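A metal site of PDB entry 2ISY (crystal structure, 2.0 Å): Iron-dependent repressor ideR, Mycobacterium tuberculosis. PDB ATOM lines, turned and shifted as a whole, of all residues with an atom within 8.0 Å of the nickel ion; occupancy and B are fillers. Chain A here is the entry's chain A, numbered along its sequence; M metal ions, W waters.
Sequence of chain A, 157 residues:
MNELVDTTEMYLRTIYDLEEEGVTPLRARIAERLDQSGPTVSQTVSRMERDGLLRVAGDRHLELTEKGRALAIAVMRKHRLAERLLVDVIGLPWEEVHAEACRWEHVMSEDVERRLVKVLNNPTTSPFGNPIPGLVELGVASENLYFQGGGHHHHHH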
ATOM      1  N   GLU A   3     -11.075   7.817 -11.443  1.00  0.00           N
ATOM      2  CA  GLU A   3     -12.431   7.684 -10.947  1.00  0.00           C
ATOM      3  C   GLU A   3     -13.522   8.252 -11.871  1.00  0.00           C
ATOM      4  O   GLU A   3     -14.642   7.754 -11.871  1.00  0.00           O
ATOM      5  CB  GLU A   3     -12.570   8.283  -9.550  1.00  0.00           C
ATOM      6  CG  GLU A   3     -12.128   7.320  -8.468  1.00  0.00           C
ATOM      7  CD  GLU A   3     -13.007   7.396  -7.224  1.00  0.00           C
ATOM      8  OE1 GLU A   3     -14.218   7.046  -7.315  1.00  0.00           O
ATOM      9  OE2 GLU A   3     -12.495   7.790  -6.152  1.00  0.00           O
ATOM     10  N   LEU A   4     -13.184   9.278 -12.655  1.00  0.00           N
ATOM     11  CA  LEU A   4     -14.135   9.895 -13.573  1.00  0.00           C
ATOM     12  C   LEU A   4     -14.315   9.042 -14.799  1.00  0.00           C
ATOM     13  O   LEU A   4     -15.290   9.205 -15.546  1.00  0.00           O
ATOM     14  CB  LEU A   4     -13.632  11.283 -13.971  1.00  0.00           C
ATOM     15  CG  LEU A   4     -13.468  12.262 -12.798  1.00  0.00           C
ATOM     16  CD1 LEU A   4     -13.092  13.652 -13.296  1.00  0.00           C
ATOM     17  CD2 LEU A   4     -14.742  12.306 -12.007  1.00  0.00           C
ATOM     18  N   VAL A   5     -13.373   8.127 -14.996  1.00  0.00           N
ATOM     19  CA  VAL A   5     -13.358   7.225 -16.131  1.00  0.00           C
ATOM     20  C   VAL A   5     -12.954   7.930 -17.424  1.00  0.00           C
ATOM     21  O   VAL A   5     -12.006   7.518 -18.106  1.00  0.00           O
ATOM     22  CB  VAL A   5     -14.718   6.490 -16.310  1.00  0.00           C
ATOM     23  CG1 VAL A   5     -14.632   5.515 -17.440  1.00  0.00           C
ATOM     24  CG2 VAL A   5     -15.097   5.755 -15.021  1.00  0.00           C
ATOM     25  N   ASP A   6     -13.668   8.991 -17.771  1.00  0.00           N
ATOM     26  CA  ASP A   6     -13.270   9.858 -18.883  1.00  0.00           C
ATOM     27  C   ASP A   6     -13.483  11.291 -18.393  1.00  0.00           C
ATOM     28  O   ASP A   6     -14.610  11.742 -18.219  1.00  0.00           O
ATOM     29  CB  ASP A   6     -14.084   9.542 -20.127  1.00  0.00           C
ATOM     30  CG  ASP A   6     -13.654  10.345 -21.330  1.00  0.00           C
ATOM     31  OD1 ASP A   6     -13.642   9.776 -22.432  1.00  0.00           O
ATOM     32  OD2 ASP A   6     -13.340  11.554 -21.195  1.00  0.00           O
ATOM     33  N   THR A   7     -12.376  11.985 -18.127  1.00  0.00           N
ATOM     34  CA  THR A   7     -12.388  13.289 -17.510  1.00  0.00           C
ATOM     35  C   THR A   7     -13.048  14.320 -18.431  1.00  0.00           C
ATOM     36  O   THR A   7     -13.874  15.150 -18.012  1.00  0.00           O
ATOM     37  CB  THR A   7     -10.919  13.732 -17.163  1.00  0.00           C
ATOM     38  OG1 THR A   7     -10.357  12.825 -16.213  1.00  0.00           O
ATOM     39  CG2 THR A   7     -10.902  15.128 -16.556  1.00  0.00           C
ATOM     40  N   GLU A   9     -15.244  13.798 -20.866  1.00  0.00           N
ATOM     41  CA  GLU A   9     -16.679  13.579 -20.974  1.00  0.00           C
ATOM     42  C   GLU A   9     -17.414  14.049 -19.730  1.00  0.00           C
ATOM     43  O   GLU A   9     -18.554  14.507 -19.830  1.00  0.00           O
ATOM     44  CB  GLU A   9     -17.020  12.115 -21.289  1.00  0.00           C
ATOM     45  CG  GLU A   9     -16.728  11.690 -22.734  1.00  0.00           C
ATOM     46  CD  GLU A   9     -17.108  10.248 -22.981  1.00  0.00           C
ATOM     47  OE1 GLU A   9     -17.362   9.472 -22.007  1.00  0.00           O
ATOM     48  OE2 GLU A   9     -17.160   9.871 -24.139  1.00  0.00           O
ATOM     49  N   MET A  10     -16.763  13.926 -18.558  1.00  0.00           N
ATOM     50  CA  MET A  10     -17.329  14.431 -17.307  1.00  0.00           C
ATOM     51  C   MET A  10     -17.363  15.972 -17.209  1.00  0.00           C
ATOM     52  O   MET A  10     -18.307  16.538 -16.650  1.00  0.00           O
ATOM     53  CB  MET A  10     -16.678  13.779 -16.104  1.00  0.00           C
ATOM     54  CG  MET A  10     -17.091  12.341 -15.903  1.00  0.00           C
ATOM     55  SD  MET A  10     -18.901  12.210 -15.806  1.00  0.00           S
ATOM     56  CE  MET A  10     -19.168  13.200 -14.321  1.00  0.00           C
ATOM     57  N   TYR A  11     -16.362  16.669 -17.742  1.00  0.00           N
ATOM     58  CA  TYR A  11     -16.453  18.134 -17.869  1.00  0.00           C
ATOM     59  C   TYR A  11     -17.602  18.485 -18.800  1.00  0.00           C
ATOM     60  O   TYR A  11     -18.427  19.345 -18.477  1.00  0.00           O
ATOM     61  CB  TYR A  11     -15.151  18.746 -18.363  1.00  0.00           C
ATOM     62  CG  TYR A  11     -14.113  18.987 -17.281  1.00  0.00           C
ATOM     63  CD1 TYR A  11     -13.713  17.971 -16.415  1.00  0.00           C
ATOM     64  CD2 TYR A  11     -13.528  20.246 -17.122  1.00  0.00           C
ATOM     65  CE1 TYR A  11     -12.755  18.186 -15.426  1.00  0.00           C
ATOM     66  CE2 TYR A  11     -12.580  20.467 -16.141  1.00  0.00           C
ATOM     67  CZ  TYR A  11     -12.206  19.447 -15.296  1.00  0.00           C
ATOM     68  OH  TYR A  11     -11.258  19.682 -14.318  1.00  0.00           O
ATOM     69  N   ARG A  13     -20.345  16.620 -19.491  1.00  0.00           N
ATOM     70  CA  ARG A  13     -21.617  16.280 -18.833  1.00  0.00           C
ATOM     71  C   ARG A  13     -21.916  17.231 -17.671  1.00  0.00           C
ATOM     72  O   ARG A  13     -23.072  17.509 -17.392  1.00  0.00           O
ATOM     73  CB  ARG A  13     -21.686  14.794 -18.351  1.00  0.00           C
ATOM     74  CG  ARG A  13     -22.981  14.034 -18.844  1.00  0.00           C
ATOM     75  CD  ARG A  13     -23.653  13.073 -17.824  1.00  0.00           C
ATOM     76  NE  ARG A  13     -23.705  13.705 -16.505  1.00  0.00           N
ATOM     77  CZ  ARG A  13     -23.246  13.156 -15.382  1.00  0.00           C
ATOM     78  NH1 ARG A  13     -22.775  11.917 -15.348  1.00  0.00           N
ATOM     79  NH2 ARG A  13     -23.289  13.867 -14.263  1.00  0.00           N
ATOM     80  N   THR A  14     -20.886  17.743 -17.009  1.00  0.00           N
ATOM     81  CA  THR A  14     -21.116  18.667 -15.894  1.00  0.00           C
ATOM     82  C   THR A  14     -21.678  20.000 -16.409  1.00  0.00           C
ATOM     83  O   THR A  14     -22.593  20.558 -15.816  1.00  0.00           O
ATOM     84  CB  THR A  14     -19.860  18.883 -15.005  1.00  0.00           C
ATOM     85  OG1 THR A  14     -19.402  17.615 -14.536  1.00  0.00           O
ATOM     86  CG2 THR A  14     -20.213  19.742 -13.800  1.00  0.00           C
ATOM     87  N   LEU A  34     -16.826  17.885  -9.434  1.00  0.00           N
ATOM     88  CA  LEU A  34     -15.847  16.816  -9.704  1.00  0.00           C
ATOM     89  C   LEU A  34     -14.670  16.702  -8.712  1.00  0.00           C
ATOM     90  O   LEU A  34     -13.752  15.900  -8.922  1.00  0.00           O
ATOM     91  CB  LEU A  34     -15.334  16.888 -11.139  1.00  0.00           C
ATOM     92  CG  LEU A  34     -16.380  16.912 -12.271  1.00  0.00           C
ATOM     93  CD1 LEU A  34     -15.736  16.978 -13.652  1.00  0.00           C
ATOM     94  CD2 LEU A  34     -17.372  15.741 -12.157  1.00  0.00           C
ATOM     95  N   VAL A  75     -23.153  11.659 -24.258  1.00  0.00           N
ATOM     96  CA  VAL A  75     -22.822  11.089 -22.941  1.00  0.00           C
ATOM     97  C   VAL A  75     -24.100  11.064 -22.067  1.00  0.00           C
ATOM     98  O   VAL A  75     -24.356  10.089 -21.340  1.00  0.00           O
ATOM     99  CB  VAL A  75     -21.718  11.923 -22.189  1.00  0.00           C
ATOM    100  CG1 VAL A  75     -21.432  11.360 -20.741  1.00  0.00           C
ATOM    101  CG2 VAL A  75     -20.448  11.918 -22.998  1.00  0.00           C
ATOM    102  N   HIS A  79     -25.989   7.978 -20.413  1.00  0.00           N
ATOM    103  CA  HIS A  79     -26.188   7.995 -18.970  1.00  0.00           C
ATOM    104  C   HIS A  79     -27.643   7.594 -18.619  1.00  0.00           C
ATOM    105  O   HIS A  79     -27.875   6.746 -17.739  1.00  0.00           O
ATOM    106  CB  HIS A  79     -25.904   9.401 -18.428  1.00  0.00           C
ATOM    107  CG  HIS A  79     -26.088   9.519 -16.956  1.00  0.00           C
ATOM    108  ND1 HIS A  79     -25.161   9.079 -16.052  1.00  0.00           N
ATOM    109  CD2 HIS A  79     -27.101  10.051 -16.225  1.00  0.00           C
ATOM    110  CE1 HIS A  79     -25.574   9.308 -14.824  1.00  0.00           C
ATOM    111  NE2 HIS A  79     -26.746   9.907 -14.906  1.00  0.00           N
ATOM    112  N   HIS A  98     -27.557   6.034 -10.251  1.00  0.00           N
ATOM    113  CA  HIS A  98     -26.804   7.195 -10.802  1.00  0.00           C
ATOM    114  C   HIS A  98     -25.279   7.025 -10.744  1.00  0.00           C
ATOM    115  O   HIS A  98     -24.573   7.289 -11.736  1.00  0.00           O
ATOM    116  CB  HIS A  98     -27.175   8.540 -10.168  1.00  0.00           C
ATOM    117  CG  HIS A  98     -26.274   9.652 -10.631  1.00  0.00           C
ATOM    118  ND1 HIS A  98     -26.454  10.302 -11.831  1.00  0.00           N
ATOM    119  CD2 HIS A  98     -25.132  10.158 -10.085  1.00  0.00           C
ATOM    120  CE1 HIS A  98     -25.486  11.186 -11.999  1.00  0.00           C
ATOM    121  NE2 HIS A  98     -24.655  11.104 -10.959  1.00  0.00           N
ATOM    122  N   ALA A  99     -24.779   6.621  -9.580  1.00  0.00           N
ATOM    123  CA  ALA A  99     -23.365   6.364  -9.399  1.00  0.00           C
ATOM    124  C   ALA A  99     -22.873   5.343 -10.432  1.00  0.00           C
ATOM    125  O   ALA A  99     -21.802   5.516 -11.010  1.00  0.00           O
ATOM    126  CB  ALA A  99     -23.080   5.845  -7.982  1.00  0.00           C
ATOM    127  N   GLU A 100     -23.638   4.268 -10.628  1.00  0.00           N
ATOM    128  CA  GLU A 100     -23.227   3.231 -11.577  1.00  0.00           C
ATOM    129  C   GLU A 100     -23.219   3.802 -13.023  1.00  0.00           C
ATOM    130  O   GLU A 100     -22.255   3.641 -13.786  1.00  0.00           O
ATOM    131  CB  GLU A 100     -24.167   2.006 -11.508  1.00  0.00           C
ATOM    132  CG  GLU A 100     -23.636   0.819 -12.368  1.00  0.00           C
ATOM    133  CD  GLU A 100     -22.717  -0.086 -11.544  1.00  0.00           C
ATOM    134  OE1 GLU A 100     -22.843  -0.050 -10.315  1.00  0.00           O
ATOM    135  OE2 GLU A 100     -21.911  -0.872 -12.097  1.00  0.00           O
ATOM    136  N   ALA A 101     -24.316   4.442 -13.380  1.00  0.00           N
ATOM    137  CA  ALA A 101     -24.523   5.072 -14.676  1.00  0.00           C
ATOM    138  C   ALA A 101     -23.454   6.128 -14.979  1.00  0.00           C
ATOM    139  O   ALA A 101     -23.025   6.306 -16.130  1.00  0.00           O
ATOM    140  CB  ALA A 101     -25.890   5.710 -14.700  1.00  0.00           C
ATOM    141  N   CSO A 102     -23.031   6.835 -13.943  1.00  0.00           N
ATOM    142  CA  CSO A 102     -21.911   7.788 -14.080  1.00  0.00           C
ATOM    143  CB  CSO A 102     -21.681   8.427 -12.733  1.00  0.00           C
ATOM    144  SG  CSO A 102     -20.168   9.392 -12.546  1.00  0.00           S
ATOM    145  C   CSO A 102     -20.613   7.113 -14.574  1.00  0.00           C
ATOM    146  O   CSO A 102     -19.765   7.774 -15.188  1.00  0.00           O
ATOM    147  OD  CSO A 102     -20.184  10.296 -13.828  1.00  0.00           O
ATOM    148  N   ARG A 103     -20.432   5.816 -14.298  1.00  0.00           N
ATOM    149  CA  ARG A 103     -19.297   5.104 -14.913  1.00  0.00           C
ATOM    150  C   ARG A 103     -19.651   4.573 -16.272  1.00  0.00           C
ATOM    151  O   ARG A 103     -18.873   4.707 -17.224  1.00  0.00           O
ATOM    152  CB  ARG A 103     -18.787   3.988 -13.996  1.00  0.00           C
ATOM    153  CG  ARG A 103     -18.239   4.509 -12.633  1.00  0.00           C
ATOM    154  CD  ARG A 103     -17.545   3.392 -11.809  1.00  0.00           C
ATOM    155  NE  ARG A 103     -18.440   2.254 -11.566  1.00  0.00           N
ATOM    156  CZ  ARG A 103     -19.354   2.213 -10.595  1.00  0.00           C
ATOM    157  NH1 ARG A 103     -20.159   1.181 -10.459  1.00  0.00           N
ATOM    158  NH2 ARG A 103     -19.468   3.241  -9.764  1.00  0.00           N
ATOM    159  N   TRP A 104     -20.798   3.914 -16.383  1.00  0.00           N
ATOM    160  CA  TRP A 104     -21.155   3.256 -17.626  1.00  0.00           C
ATOM    161  C   TRP A 104     -21.340   4.214 -18.810  1.00  0.00           C
ATOM    162  O   TRP A 104     -21.173   3.809 -19.970  1.00  0.00           O
ATOM    163  CB  TRP A 104     -22.449   2.461 -17.410  1.00  0.00           C
ATOM    164  CG  TRP A 104     -22.360   1.258 -16.500  1.00  0.00           C
ATOM    165  CD1 TRP A 104     -21.515   1.051 -15.430  1.00  0.00           C
ATOM    166  CD2 TRP A 104     -23.218   0.135 -16.556  1.00  0.00           C
ATOM    167  NE1 TRP A 104     -21.796  -0.183 -14.840  1.00  0.00           N
ATOM    168  CE2 TRP A 104     -22.843  -0.758 -15.525  1.00  0.00           C
ATOM    169  CE3 TRP A 104     -24.269  -0.231 -17.416  1.00  0.00           C
ATOM    170  CZ2 TRP A 104     -23.478  -1.985 -15.336  1.00  0.00           C
ATOM    171  CZ3 TRP A 104     -24.893  -1.436 -17.225  1.00  0.00           C
ATOM    172  CH2 TRP A 104     -24.497  -2.299 -16.187  1.00  0.00           C
ATOM    173  N   GLU A 105     -21.717   5.467 -18.533  1.00  0.00           N
ATOM    174  CA  GLU A 105     -21.951   6.430 -19.596  1.00  0.00           C
ATOM    175  C   GLU A 105     -20.720   6.638 -20.464  1.00  0.00           C
ATOM    176  O   GLU A 105     -20.844   7.083 -21.570  1.00  0.00           O
ATOM    177  CB  GLU A 105     -22.364   7.786 -19.012  1.00  0.00           C
ATOM    178  CG  GLU A 105     -21.317   8.430 -18.107  1.00  0.00           C
ATOM    179  CD  GLU A 105     -21.846   9.653 -17.378  1.00  0.00           C
ATOM    180  OE1 GLU A 105     -22.985  10.053 -17.677  1.00  0.00           O
ATOM    181  OE2 GLU A 105     -21.104  10.227 -16.556  1.00  0.00           O
ATOM    182  N   HIS A 106     -19.535   6.306 -19.943  1.00  0.00           N
ATOM    183  CA  HIS A 106     -18.272   6.506 -20.679  1.00  0.00           C
ATOM    184  C   HIS A 106     -17.810   5.311 -21.519  1.00  0.00           C
ATOM    185  O   HIS A 106     -16.869   5.438 -22.320  1.00  0.00           O
ATOM    186  CB  HIS A 106     -17.173   6.956 -19.691  1.00  0.00           C
ATOM    187  CG  HIS A 106     -17.626   8.104 -18.835  1.00  0.00           C
ATOM    188  ND1 HIS A 106     -17.863   9.353 -19.343  1.00  0.00           N
ATOM    189  CD2 HIS A 106     -17.976   8.162 -17.522  1.00  0.00           C
ATOM    190  CE1 HIS A 106     -18.316  10.145 -18.392  1.00  0.00           C
ATOM    191  NE2 HIS A 106     -18.400   9.446 -17.275  1.00  0.00           N
HETATM  192 NI    NI M   1     -19.383   9.860 -15.508  1.00  0.00          NI
HETATM  193  O   HOH W   1     -17.661   9.641 -14.147  1.00  0.00           O
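The nickel ion is bound by OD of CSO 102, OE2 of Glu 105, NE2 of His 106, O of CSO 102, water W1 and SD of Met 10.
Water W1 lies within hydrogen-bond range of the backbone carbonyl oxygen of Leu 4 (2.8 Å) and SG of CSO 102 (3.0 Å).
Residues that only touch the nickel ion: Arg 13 (3.97 Å).
Five residues have an atom within 4 Å of the nickel ion: Met 10, Arg 13, CSO 102, Glu 105 and His 106.
The guanidinium group of Arg 13 sits close to OD of CSO 102, 3.4 Å away.
OE1 of Glu 105 is in salt-bridge range of NH1 of Arg 13 (3.0 Å).
The side-chain carboxylate (OE1) of Glu 105 lies within hydrogen-bond range of a ring nitrogen (ND1) of His 79 (2.9 Å).
A ring nitrogen (ND1) of His 106 is in hydrogen-bond range of the side-chain carboxylate of Glu 9.
The backbone carbonyl oxygen of Met 10 sits at hydrogen-bond distance from the side-chain hydroxyl of Thr 14, at 2.6 Å.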
